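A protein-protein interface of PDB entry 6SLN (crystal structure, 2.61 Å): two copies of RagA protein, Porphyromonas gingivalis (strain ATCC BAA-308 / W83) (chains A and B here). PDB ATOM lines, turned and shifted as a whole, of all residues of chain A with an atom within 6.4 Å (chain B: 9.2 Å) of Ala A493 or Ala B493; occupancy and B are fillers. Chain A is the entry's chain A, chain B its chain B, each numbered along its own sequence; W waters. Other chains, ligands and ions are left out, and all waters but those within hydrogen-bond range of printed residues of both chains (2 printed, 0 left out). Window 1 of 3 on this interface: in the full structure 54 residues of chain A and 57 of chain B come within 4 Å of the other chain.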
ATOM      1  N   THR A 469      22.774  20.264  26.626  1.00  0.00           N
ATOM      2  CA  THR A 469      23.346  21.184  27.582  1.00  0.00           C
ATOM      3  C   THR A 469      22.430  22.381  27.725  1.00  0.00           C
ATOM      4  O   THR A 469      21.987  22.958  26.728  1.00  0.00           O
ATOM      5  CB  THR A 469      24.729  21.633  27.134  1.00  0.00           C
ATOM      6  OG1 THR A 469      25.492  20.472  26.792  1.00  0.00           O
ATOM      7  CG2 THR A 469      25.422  22.425  28.243  1.00  0.00           C
ATOM      8  N   ARG A 470      22.150  22.739  28.961  1.00  0.00           N
ATOM      9  CA  ARG A 470      21.454  23.972  29.277  1.00  0.00           C
ATOM     10  C   ARG A 470      22.424  24.877  30.017  1.00  0.00           C
ATOM     11  O   ARG A 470      23.073  24.457  30.986  1.00  0.00           O
ATOM     12  CB  ARG A 470      20.203  23.698  30.120  1.00  0.00           C
ATOM     13  CG  ARG A 470      19.073  23.049  29.309  1.00  0.00           C
ATOM     14  CD  ARG A 470      18.418  24.077  28.414  1.00  0.00           C
ATOM     15  NE  ARG A 470      17.456  24.893  29.145  1.00  0.00           N
ATOM     16  CZ  ARG A 470      17.736  26.088  29.675  1.00  0.00           C
ATOM     17  NH1 ARG A 470      18.950  26.610  29.546  1.00  0.00           N
ATOM     18  NH2 ARG A 470      16.801  26.776  30.323  1.00  0.00           N
ATOM     19  N   THR A 471      22.561  26.096  29.538  1.00  0.00           N
ATOM     20  CA  THR A 471      23.322  27.089  30.263  1.00  0.00           C
ATOM     21  C   THR A 471      22.378  28.213  30.616  1.00  0.00           C
ATOM     22  O   THR A 471      21.388  28.468  29.916  1.00  0.00           O
ATOM     23  CB  THR A 471      24.507  27.624  29.466  1.00  0.00           C
ATOM     24  OG1 THR A 471      24.030  28.320  28.307  1.00  0.00           O
ATOM     25  CG2 THR A 471      25.368  26.485  29.053  1.00  0.00           C
ATOM     26  N   GLU A 491      19.249  32.258  28.343  1.00  0.00           N
ATOM     27  CA  GLU A 491      19.139  30.814  28.459  1.00  0.00           C
ATOM     28  C   GLU A 491      19.455  30.167  27.116  1.00  0.00           C
ATOM     29  O   GLU A 491      19.016  30.642  26.054  1.00  0.00           O
ATOM     30  CB  GLU A 491      17.737  30.402  28.915  1.00  0.00           C
ATOM     31  CG  GLU A 491      17.327  31.036  30.190  1.00  0.00           C
ATOM     32  CD  GLU A 491      17.801  30.258  31.386  1.00  0.00           C
ATOM     33  OE1 GLU A 491      18.079  29.053  31.239  1.00  0.00           O
ATOM     34  OE2 GLU A 491      17.886  30.856  32.480  1.00  0.00           O
ATOM     35  N   ARG A 492      20.182  29.059  27.167  1.00  0.00           N
ATOM     36  CA  ARG A 492      20.664  28.431  25.955  1.00  0.00           C
ATOM     37  C   ARG A 492      20.459  26.937  26.042  1.00  0.00           C
ATOM     38  O   ARG A 492      20.542  26.342  27.125  1.00  0.00           O
ATOM     39  CB  ARG A 492      22.153  28.711  25.729  1.00  0.00           C
ATOM     40  CG  ARG A 492      22.415  29.967  24.951  1.00  0.00           C
ATOM     41  CD  ARG A 492      23.829  30.319  25.099  1.00  0.00           C
ATOM     42  NE  ARG A 492      24.141  31.592  24.468  1.00  0.00           N
ATOM     43  CZ  ARG A 492      25.302  32.212  24.638  1.00  0.00           C
ATOM     44  NH1 ARG A 492      26.217  31.656  25.416  1.00  0.00           N
ATOM     45  NH2 ARG A 492      25.543  33.368  24.035  1.00  0.00           N
ATOM     46  N   ALA A 493      20.242  26.329  24.879  1.00  0.00           N
ATOM     47  CA  ALA A 493      20.079  24.887  24.783  1.00  0.00           C
ATOM     48  C   ALA A 493      20.911  24.405  23.618  1.00  0.00           C
ATOM     49  O   ALA A 493      20.710  24.861  22.489  1.00  0.00           O
ATOM     50  CB  ALA A 493      18.609  24.506  24.598  1.00  0.00           C
ATOM     51  N   TYR A 494      21.849  23.500  23.900  1.00  0.00           N
ATOM     52  CA  TYR A 494      22.774  22.931  22.926  1.00  0.00           C
ATOM     53  C   TYR A 494      22.443  21.462  22.757  1.00  0.00           C
ATOM     54  O   TYR A 494      22.117  20.785  23.745  1.00  0.00           O
ATOM     55  CB  TYR A 494      24.242  23.026  23.400  1.00  0.00           C
ATOM     56  CG  TYR A 494      24.819  24.403  23.684  1.00  0.00           C
ATOM     57  CD1 TYR A 494      24.550  25.072  24.875  1.00  0.00           C
ATOM     58  CD2 TYR A 494      25.695  25.002  22.786  1.00  0.00           C
ATOM     59  CE1 TYR A 494      25.104  26.328  25.131  1.00  0.00           C
ATOM     60  CE2 TYR A 494      26.251  26.243  23.037  1.00  0.00           C
ATOM     61  CZ  TYR A 494      25.954  26.904  24.201  1.00  0.00           C
ATOM     62  OH  TYR A 494      26.507  28.140  24.425  1.00  0.00           O
ATOM     63  N   ARG A 495      22.594  20.956  21.526  1.00  0.00           N
ATOM     64  CA  ARG A 495      22.374  19.542  21.232  1.00  0.00           C
ATOM     65  C   ARG A 495      23.421  19.009  20.268  1.00  0.00           C
ATOM     66  O   ARG A 495      23.638  19.594  19.204  1.00  0.00           O
ATOM     67  CB  ARG A 495      20.992  19.319  20.628  1.00  0.00           C
ATOM     68  CG  ARG A 495      20.761  17.901  20.198  1.00  0.00           C
ATOM     69  CD  ARG A 495      19.297  17.645  19.983  1.00  0.00           C
ATOM     70  NE  ARG A 495      18.647  17.336  21.243  1.00  0.00           N
ATOM     71  CZ  ARG A 495      17.383  16.956  21.359  1.00  0.00           C
ATOM     72  NH1 ARG A 495      16.609  16.812  20.288  1.00  0.00           N
ATOM     73  NH2 ARG A 495      16.913  16.694  22.555  1.00  0.00           N
ATOM     74  N   ASP A 531      23.174  21.667  17.161  1.00  0.00           N
ATOM     75  CA  ASP A 531      22.649  23.023  17.109  1.00  0.00           C
ATOM     76  C   ASP A 531      22.770  23.684  18.469  1.00  0.00           C
ATOM     77  O   ASP A 531      23.178  23.069  19.457  1.00  0.00           O
ATOM     78  CB  ASP A 531      21.197  23.056  16.608  1.00  0.00           C
ATOM     79  CG  ASP A 531      20.202  22.495  17.611  1.00  0.00           C
ATOM     80  OD1 ASP A 531      20.602  21.742  18.518  1.00  0.00           O
ATOM     81  OD2 ASP A 531      19.000  22.793  17.474  1.00  0.00           O
ATOM     82  N   VAL A 532      22.442  24.970  18.490  1.00  0.00           N
ATOM     83  CA  VAL A 532      22.267  25.705  19.730  1.00  0.00           C
ATOM     84  C   VAL A 532      21.174  26.730  19.472  1.00  0.00           C
ATOM     85  O   VAL A 532      21.047  27.260  18.363  1.00  0.00           O
ATOM     86  CB  VAL A 532      23.600  26.359  20.220  1.00  0.00           C
ATOM     87  CG1 VAL A 532      24.289  27.147  19.109  1.00  0.00           C
ATOM     88  CG2 VAL A 532      23.382  27.281  21.424  1.00  0.00           C
ATOM     89  N   ILE A 533      20.367  26.983  20.496  1.00  0.00           N
ATOM     90  CA  ILE A 533      19.397  28.069  20.496  1.00  0.00           C
ATOM     91  C   ILE A 533      19.533  28.800  21.815  1.00  0.00           C
ATOM     92  O   ILE A 533      19.955  28.232  22.832  1.00  0.00           O
ATOM     93  CB  ILE A 533      17.938  27.603  20.322  1.00  0.00           C
ATOM     94  CG1 ILE A 533      17.495  26.795  21.555  1.00  0.00           C
ATOM     95  CG2 ILE A 533      17.783  26.827  19.038  1.00  0.00           C
ATOM     96  CD1 ILE A 533      16.084  26.183  21.448  1.00  0.00           C
ATOM     97  N   GLY A 534      19.185  30.073  21.789  1.00  0.00           N
ATOM     98  CA  GLY A 534      19.360  30.863  22.974  1.00  0.00           C
ATOM     99  C   GLY A 534      18.387  32.004  22.945  1.00  0.00           C
ATOM    100  O   GLY A 534      18.169  32.600  21.892  1.00  0.00           O
ATOM    101  N   GLU B 438      11.956  15.917  18.859  1.00  0.00           N
ATOM    102  CA  GLU B 438      12.834  14.792  19.153  1.00  0.00           C
ATOM    103  C   GLU B 438      13.136  14.834  20.641  1.00  0.00           C
ATOM    104  O   GLU B 438      13.736  15.798  21.127  1.00  0.00           O
ATOM    105  CB  GLU B 438      14.112  14.824  18.317  1.00  0.00           C
ATOM    106  CG  GLU B 438      14.956  13.590  18.538  1.00  0.00           C
ATOM    107  CD  GLU B 438      15.864  13.250  17.380  1.00  0.00           C
ATOM    108  OE1 GLU B 438      15.364  13.156  16.231  1.00  0.00           O
ATOM    109  OE2 GLU B 438      17.075  13.056  17.632  1.00  0.00           O
ATOM    110  N   THR B 467      14.653  13.663  30.594  1.00  0.00           N
ATOM    111  CA  THR B 467      14.037  13.976  29.313  1.00  0.00           C
ATOM    112  C   THR B 467      14.598  15.296  28.811  1.00  0.00           C
ATOM    113  O   THR B 467      14.510  16.316  29.506  1.00  0.00           O
ATOM    114  CB  THR B 467      12.515  14.079  29.444  1.00  0.00           C
ATOM    115  OG1 THR B 467      12.016  12.961  30.190  1.00  0.00           O
ATOM    116  CG2 THR B 467      11.872  14.127  28.069  1.00  0.00           C
ATOM    117  N   ASN B 468      15.163  15.285  27.605  1.00  0.00           N
ATOM    118  CA  ASN B 468      15.499  16.511  26.887  1.00  0.00           C
ATOM    119  C   ASN B 468      14.764  16.468  25.565  1.00  0.00           C
ATOM    120  O   ASN B 468      14.977  15.547  24.770  1.00  0.00           O
ATOM    121  CB  ASN B 468      17.006  16.666  26.665  1.00  0.00           C
ATOM    122  CG  ASN B 468      17.711  17.183  27.895  1.00  0.00           C
ATOM    123  OD1 ASN B 468      17.693  18.386  28.180  1.00  0.00           O
ATOM    124  ND2 ASN B 468      18.291  16.273  28.664  1.00  0.00           N
ATOM    125  N   THR B 469      13.896  17.447  25.339  1.00  0.00           N
ATOM    126  CA  THR B 469      13.044  17.462  24.158  1.00  0.00           C
ATOM    127  C   THR B 469      13.198  18.782  23.416  1.00  0.00           C
ATOM    128  O   THR B 469      13.021  19.861  23.991  1.00  0.00           O
ATOM    129  CB  THR B 469      11.576  17.221  24.544  1.00  0.00           C
ATOM    130  OG1 THR B 469      11.486  16.045  25.363  1.00  0.00           O
ATOM    131  CG2 THR B 469      10.742  17.025  23.312  1.00  0.00           C
ATOM    132  N   ARG B 470      13.524  18.686  22.140  1.00  0.00           N
ATOM    133  CA  ARG B 470      13.605  19.830  21.247  1.00  0.00           C
ATOM    134  C   ARG B 470      12.451  19.746  20.254  1.00  0.00           C
ATOM    135  O   ARG B 470      12.177  18.670  19.713  1.00  0.00           O
ATOM    136  CB  ARG B 470      14.943  19.824  20.516  1.00  0.00           C
ATOM    137  CG  ARG B 470      16.106  20.265  21.364  1.00  0.00           C
ATOM    138  CD  ARG B 470      16.039  21.777  21.602  1.00  0.00           C
ATOM    139  NE  ARG B 470      16.525  22.523  20.439  1.00  0.00           N
ATOM    140  CZ  ARG B 470      15.753  23.232  19.617  1.00  0.00           C
ATOM    141  NH1 ARG B 470      14.442  23.307  19.806  1.00  0.00           N
ATOM    142  NH2 ARG B 470      16.292  23.871  18.598  1.00  0.00           N
ATOM    143  N   THR B 471      11.756  20.865  20.040  1.00  0.00           N
ATOM    144  CA  THR B 471      10.662  20.921  19.082  1.00  0.00           C
ATOM    145  C   THR B 471      10.833  22.128  18.186  1.00  0.00           C
ATOM    146  O   THR B 471      11.103  23.239  18.661  1.00  0.00           O
ATOM    147  CB  THR B 471       9.282  21.059  19.722  1.00  0.00           C
ATOM    148  OG1 THR B 471       9.209  22.349  20.344  1.00  0.00           O
ATOM    149  CG2 THR B 471       9.008  19.954  20.714  1.00  0.00           C
ATOM    150  N   SER B 472      10.611  21.915  16.899  1.00  0.00           N
ATOM    151  CA  SER B 472      10.728  22.974  15.917  1.00  0.00           C
ATOM    152  C   SER B 472       9.411  23.113  15.175  1.00  0.00           C
ATOM    153  O   SER B 472       8.795  22.117  14.779  1.00  0.00           O
ATOM    154  CB  SER B 472      11.857  22.694  14.933  1.00  0.00           C
ATOM    155  OG  SER B 472      12.248  23.898  14.306  1.00  0.00           O
ATOM    156  N   ARG B 490       9.549  28.820  15.581  1.00  0.00           N
ATOM    157  CA  ARG B 490       9.613  28.728  17.040  1.00  0.00           C
ATOM    158  C   ARG B 490      10.387  27.479  17.435  1.00  0.00           C
ATOM    159  O   ARG B 490      10.131  26.380  16.921  1.00  0.00           O
ATOM    160  CB  ARG B 490       8.218  28.723  17.689  1.00  0.00           C
ATOM    161  CG  ARG B 490       8.225  28.678  19.215  1.00  0.00           C
ATOM    162  CD  ARG B 490       6.870  29.034  19.806  1.00  0.00           C
ATOM    163  NE  ARG B 490       5.859  28.105  19.331  1.00  0.00           N
ATOM    164  CZ  ARG B 490       4.855  28.445  18.529  1.00  0.00           C
ATOM    165  NH1 ARG B 490       4.730  29.708  18.132  1.00  0.00           N
ATOM    166  NH2 ARG B 490       3.978  27.524  18.124  1.00  0.00           N
ATOM    167  N   GLU B 491      11.342  27.672  18.339  1.00  0.00           N
ATOM    168  CA  GLU B 491      12.198  26.623  18.856  1.00  0.00           C
ATOM    169  C   GLU B 491      11.990  26.517  20.365  1.00  0.00           C
ATOM    170  O   GLU B 491      11.818  27.529  21.059  1.00  0.00           O
ATOM    171  CB  GLU B 491      13.669  26.913  18.512  1.00  0.00           C
ATOM    172  CG  GLU B 491      13.923  27.006  17.011  1.00  0.00           C
ATOM    173  CD  GLU B 491      13.926  25.640  16.343  1.00  0.00           C
ATOM    174  OE1 GLU B 491      14.402  24.679  16.974  1.00  0.00           O
ATOM    175  OE2 GLU B 491      13.470  25.526  15.187  1.00  0.00           O
ATOM    176  N   ARG B 492      12.004  25.282  20.860  1.00  0.00           N
ATOM    177  CA  ARG B 492      11.706  24.988  22.248  1.00  0.00           C
ATOM    178  C   ARG B 492      12.628  23.905  22.763  1.00  0.00           C
ATOM    179  O   ARG B 492      12.861  22.895  22.086  1.00  0.00           O
ATOM    180  CB  ARG B 492      10.276  24.505  22.428  1.00  0.00           C
ATOM    181  CG  ARG B 492       9.316  25.566  22.785  1.00  0.00           C
ATOM    182  CD  ARG B 492       7.927  25.057  22.634  1.00  0.00           C
ATOM    183  NE  ARG B 492       6.988  26.160  22.705  1.00  0.00           N
ATOM    184  CZ  ARG B 492       5.718  26.044  22.372  1.00  0.00           C
ATOM    185  NH1 ARG B 492       5.289  24.863  21.948  1.00  0.00           N
ATOM    186  NH2 ARG B 492       4.905  27.096  22.456  1.00  0.00           N
ATOM    187  N   ALA B 493      13.114  24.095  23.984  1.00  0.00           N
ATOM    188  CA  ALA B 493      13.893  23.065  24.653  1.00  0.00           C
ATOM    189  C   ALA B 493      13.220  22.732  25.971  1.00  0.00           C
ATOM    190  O   ALA B 493      12.986  23.626  26.794  1.00  0.00           O
ATOM    191  CB  ALA B 493      15.332  23.513  24.861  1.00  0.00           C
ATOM    192  N   TYR B 494      12.889  21.454  26.150  1.00  0.00           N
ATOM    193  CA  TYR B 494      12.260  20.939  27.359  1.00  0.00           C
ATOM    194  C   TYR B 494      13.278  20.115  28.129  1.00  0.00           C
ATOM    195  O   TYR B 494      13.961  19.265  27.539  1.00  0.00           O
ATOM    196  CB  TYR B 494      11.049  20.054  27.036  1.00  0.00           C
ATOM    197  CG  TYR B 494       9.853  20.737  26.422  1.00  0.00           C
ATOM    198  CD1 TYR B 494       9.781  20.926  25.055  1.00  0.00           C
ATOM    199  CD2 TYR B 494       8.757  21.118  27.188  1.00  0.00           C
ATOM    200  CE1 TYR B 494       8.683  21.515  24.457  1.00  0.00           C
ATOM    201  CE2 TYR B 494       7.648  21.725  26.593  1.00  0.00           C
ATOM    202  CZ  TYR B 494       7.626  21.915  25.220  1.00  0.00           C
ATOM    203  OH  TYR B 494       6.564  22.505  24.575  1.00  0.00           O
ATOM    204  N   ARG B 495      13.335  20.326  29.452  1.00  0.00           N
ATOM    205  CA  ARG B 495      14.160  19.513  30.339  1.00  0.00           C
ATOM    206  C   ARG B 495      13.339  19.016  31.517  1.00  0.00           C
ATOM    207  O   ARG B 495      12.716  19.808  32.231  1.00  0.00           O
ATOM    208  CB  ARG B 495      15.382  20.286  30.855  1.00  0.00           C
ATOM    209  CG  ARG B 495      16.192  19.479  31.842  1.00  0.00           C
ATOM    210  CD  ARG B 495      17.571  20.021  31.967  1.00  0.00           C
ATOM    211  NE  ARG B 495      18.383  19.549  30.866  1.00  0.00           N
ATOM    212  CZ  ARG B 495      19.671  19.815  30.743  1.00  0.00           C
ATOM    213  NH1 ARG B 495      20.282  20.535  31.673  1.00  0.00           N
ATOM    214  NH2 ARG B 495      20.342  19.351  29.704  1.00  0.00           N
ATOM    215  N   ASP B 496      13.365  17.705  31.726  1.00  0.00           N
ATOM    216  CA  ASP B 496      12.715  17.059  32.854  1.00  0.00           C
ATOM    217  C   ASP B 496      13.750  16.177  33.509  1.00  0.00           C
ATOM    218  O   ASP B 496      14.262  15.249  32.871  1.00  0.00           O
ATOM    219  CB  ASP B 496      11.525  16.193  32.430  1.00  0.00           C
ATOM    220  CG  ASP B 496      10.414  16.986  31.807  1.00  0.00           C
ATOM    221  OD1 ASP B 496       9.997  17.994  32.408  1.00  0.00           O
ATOM    222  OD2 ASP B 496       9.935  16.590  30.722  1.00  0.00           O
ATOM    223  N   GLY B 530      11.677  20.575  36.436  1.00  0.00           N
ATOM    224  CA  GLY B 530      11.311  20.637  35.043  1.00  0.00           C
ATOM    225  C   GLY B 530      11.406  22.047  34.498  1.00  0.00           C
ATOM    226  O   GLY B 530      11.299  23.031  35.226  1.00  0.00           O
ATOM    227  N   ASP B 531      11.515  22.117  33.175  1.00  0.00           N
ATOM    228  CA  ASP B 531      12.097  23.257  32.489  1.00  0.00           C
ATOM    229  C   ASP B 531      11.529  23.347  31.081  1.00  0.00           C
ATOM    230  O   ASP B 531      11.502  22.338  30.378  1.00  0.00           O
ATOM    231  CB  ASP B 531      13.614  23.057  32.411  1.00  0.00           C
ATOM    232  CG  ASP B 531      14.337  24.290  32.031  1.00  0.00           C
ATOM    233  OD1 ASP B 531      13.675  25.324  31.872  1.00  0.00           O
ATOM    234  OD2 ASP B 531      15.575  24.230  31.915  1.00  0.00           O
ATOM    235  N   VAL B 532      11.129  24.535  30.642  1.00  0.00           N
ATOM    236  CA  VAL B 532      11.002  24.744  29.201  1.00  0.00           C
ATOM    237  C   VAL B 532      11.348  26.183  28.855  1.00  0.00           C
ATOM    238  O   VAL B 532      10.976  27.124  29.568  1.00  0.00           O
ATOM    239  CB  VAL B 532       9.600  24.376  28.661  1.00  0.00           C
ATOM    240  CG1 VAL B 532       8.496  25.202  29.345  1.00  0.00           C
ATOM    241  CG2 VAL B 532       9.576  24.580  27.157  1.00  0.00           C
ATOM    242  N   ILE B 533      12.068  26.343  27.745  1.00  0.00           N
ATOM    243  CA  ILE B 533      12.365  27.644  27.168  1.00  0.00           C
ATOM    244  C   ILE B 533      11.987  27.599  25.702  1.00  0.00           C
ATOM    245  O   ILE B 533      12.066  26.556  25.041  1.00  0.00           O
ATOM    246  CB  ILE B 533      13.844  28.045  27.339  1.00  0.00           C
ATOM    247  CG1 ILE B 533      14.757  27.094  26.553  1.00  0.00           C
ATOM    248  CG2 ILE B 533      14.225  28.097  28.818  1.00  0.00           C
ATOM    249  CD1 ILE B 533      16.220  27.478  26.598  1.00  0.00           C
ATOM    250  N   GLY B 534      11.552  28.736  25.200  1.00  0.00           N
ATOM    251  CA  GLY B 534      11.077  28.812  23.835  1.00  0.00           C
ATOM    252  C   GLY B 534      11.418  30.175  23.306  1.00  0.00           C
ATOM    253  O   GLY B 534      11.444  31.157  24.056  1.00  0.00           O
ATOM    254  N   ALA B 535      11.736  30.234  22.011  1.00  0.00           N
ATOM    255  CA  ALA B 535      11.950  31.506  21.344  1.00  0.00           C
ATOM    256  C   ALA B 535      11.358  31.407  19.957  1.00  0.00           C
ATOM    257  O   ALA B 535      11.229  30.311  19.410  1.00  0.00           O
ATOM    258  CB  ALA B 535      13.435  31.889  21.264  1.00  0.00           C
ATOM    259  N   LEU B 548      16.650  31.511  13.660  1.00  0.00           N
ATOM    260  CA  LEU B 548      15.985  32.441  14.561  1.00  0.00           C
ATOM    261  C   LEU B 548      16.667  33.794  14.570  1.00  0.00           C
ATOM    262  O   LEU B 548      15.997  34.833  14.591  1.00  0.00           O
ATOM    263  CB  LEU B 548      15.928  31.869  15.972  1.00  0.00           C
ATOM    264  CG  LEU B 548      14.865  30.781  16.131  1.00  0.00           C
ATOM    265  CD1 LEU B 548      14.753  30.450  17.592  1.00  0.00           C
ATOM    266  CD2 LEU B 548      13.521  31.230  15.573  1.00  0.00           C
ATOM    267  N   GLU B 561       9.529  32.228  25.661  1.00  0.00           N
ATOM    268  CA  GLU B 561       8.793  31.410  26.600  1.00  0.00           C
ATOM    269  C   GLU B 561       9.728  30.869  27.675  1.00  0.00           C
ATOM    270  O   GLU B 561      10.885  30.534  27.406  1.00  0.00           O
ATOM    271  CB  GLU B 561       8.108  30.253  25.881  1.00  0.00           C
ATOM    272  CG  GLU B 561       7.063  30.672  24.909  1.00  0.00           C
ATOM    273  CD  GLU B 561       6.505  29.495  24.169  1.00  0.00           C
ATOM    274  OE1 GLU B 561       7.296  28.786  23.512  1.00  0.00           O
ATOM    275  OE2 GLU B 561       5.281  29.263  24.272  1.00  0.00           O
ATOM    276  N   HIS B 562       9.198  30.743  28.890  1.00  0.00           N
ATOM    277  CA  HIS B 562       9.973  30.202  30.002  1.00  0.00           C
ATOM    278  C   HIS B 562       9.027  29.707  31.091  1.00  0.00           C
ATOM    279  O   HIS B 562       8.268  30.499  31.647  1.00  0.00           O
ATOM    280  CB  HIS B 562      10.910  31.286  30.545  1.00  0.00           C
ATOM    281  CG  HIS B 562      12.020  30.744  31.380  1.00  0.00           C
ATOM    282  ND1 HIS B 562      12.970  31.548  31.975  1.00  0.00           N
ATOM    283  CD2 HIS B 562      12.335  29.468  31.714  1.00  0.00           C
ATOM    284  CE1 HIS B 562      13.825  30.788  32.636  1.00  0.00           C
ATOM    285  NE2 HIS B 562      13.458  29.523  32.499  1.00  0.00           N
ATOM    286  N   ARG B 563       9.070  28.416  31.406  1.00  0.00           N
ATOM    287  CA  ARG B 563       8.351  27.867  32.547  1.00  0.00           C
ATOM    288  C   ARG B 563       9.269  26.932  33.332  1.00  0.00           C
ATOM    289  O   ARG B 563      10.092  26.206  32.753  1.00  0.00           O
ATOM    290  CB  ARG B 563       7.051  27.104  32.128  1.00  0.00           C
ATOM    291  CG  ARG B 563       5.859  27.977  31.722  1.00  0.00           C
ATOM    292  CD  ARG B 563       4.651  27.156  31.165  1.00  0.00           C
ATOM    293  NE  ARG B 563       4.891  26.497  29.870  1.00  0.00           N
ATOM    294  CZ  ARG B 563       4.796  27.090  28.672  1.00  0.00           C
ATOM    295  NH1 ARG B 563       4.467  28.377  28.583  1.00  0.00           N
ATOM    296  NH2 ARG B 563       5.035  26.400  27.555  1.00  0.00           N
HETATM  297  O   HOH W   1      19.438  22.685  21.013  1.00  0.00           O
HETATM  298  O   HOH W   2      15.367  23.367  28.815  1.00  0.00           O
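NH2 of Arg A470 is in salt-bridge range of OD2 of Asp B531, 3.2 Å away.
The backbone carbonyl oxygen (O) of Glu B438 sits at hydrogen-bond distance from the guanidinium group (NH1) of Arg A495 (3.2 Å).
The guanidinium group (NH2) of Arg A495 is in hydrogen-bond range of the backbone carbonyl oxygen (O) of Asn B468 (3.2 Å).
The guanidinium group (NH2) of Arg B470 is in salt-bridge range of the side-chain carboxylate (OD2) of Asp A531 (3.1 Å).
NH2 of Arg A470 is in salt-bridge range of OE1 of Glu A491, at 2.8 Å.
The backbone NH of Asp A531 sits at hydrogen-bond distance from the backbone carbonyl oxygen of Arg A495, at 2.9 Å.
The side-chain amide oxygen of Asn B468 is in hydrogen-bond range of the guanidinium group of Arg B495 (3.0 Å).
OE1 of Glu B491 is in salt-bridge range of NH2 of Arg B470 (2.6 Å).
The backbone NH (N) of Ala B493 is in hydrogen-bond range of the backbone carbonyl oxygen (O) of Ile B533, at 2.9 Å.
N of Asp B531 lies within hydrogen-bond range of O of Arg B495, at 2.8 Å.
Among the printed residues, pairs that only touch across the chains: Arg A470 with Ile B533, Ile A533 with Arg B470, Ala A493 with Ala B493, Arg A495 with Arg B470, Arg A470 with Arg B495 and Ile A533 with Glu B491.
Ala A493 touches just one residue of chain B: Ala B493.
Ala B493 touches just one residue of chain A: Ala A493.
Printed residues of chain A within 4 Å of Arg B470: Arg A495 (3.4 Å), Asp A531 (3.1 Å) and Ile A533 (3.3 Å).
Printed residues of chain B within 4 Å of Arg A495: Glu B438 (3.2 Å), Asn B468 (3.2 Å) and Arg B470 (3.4 Å).
Printed residues of chain A within 4 Å of Asp B531: Arg A470 (3.2 Å).
Leu B548 touches none of the printed residues of chain A.
Val A532 touches none of the printed residues of chain B.
The nearest residue of chain A that does not touch Ala B493 is Ile A533 (4.4 Å).
The nearest printed residue of chain A that does not touch Glu B438 is Asp A531 (9.4 Å).
Of the 12 printed residues of chain A, 5 touch a printed residue of chain B.
Hydrophobic or aromatic side chains of chain A that line the printed part of chain B: Ala A493 and Ile A533.
Of the 24 printed residues of chain B, 8 touch a printed residue of chain A.
Printed residues of chain B that touch a printed residue of chain A: Glu B438, Asn B468, Arg B470, Glu B491, Ala B493, Arg B495, Asp B531 and Ile B533.
Among the printed residues, 10 pairs touch across the chains.
Arg A470 touches Arg B495, and with the chains exchanged Arg A495 touches Arg B470.
Arg A470 touches Asp B531, and with the chains exchanged Asp A531 touches Arg B470.
Arg A470 touches Ile B533, and with the chains exchanged Ile A533 touches Arg B470.
Ala B493 touches its own counterpart, Ala A493.
12 positions are printed for both chains.
Water W2 lies within hydrogen-bond range of NE of Arg A470, O of Ala B493 and OD2 of Asp B531.
Water W1 lies within hydrogen-bond range of OD1 of Asp A531, O of Ala A493 and NE of Arg B470.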
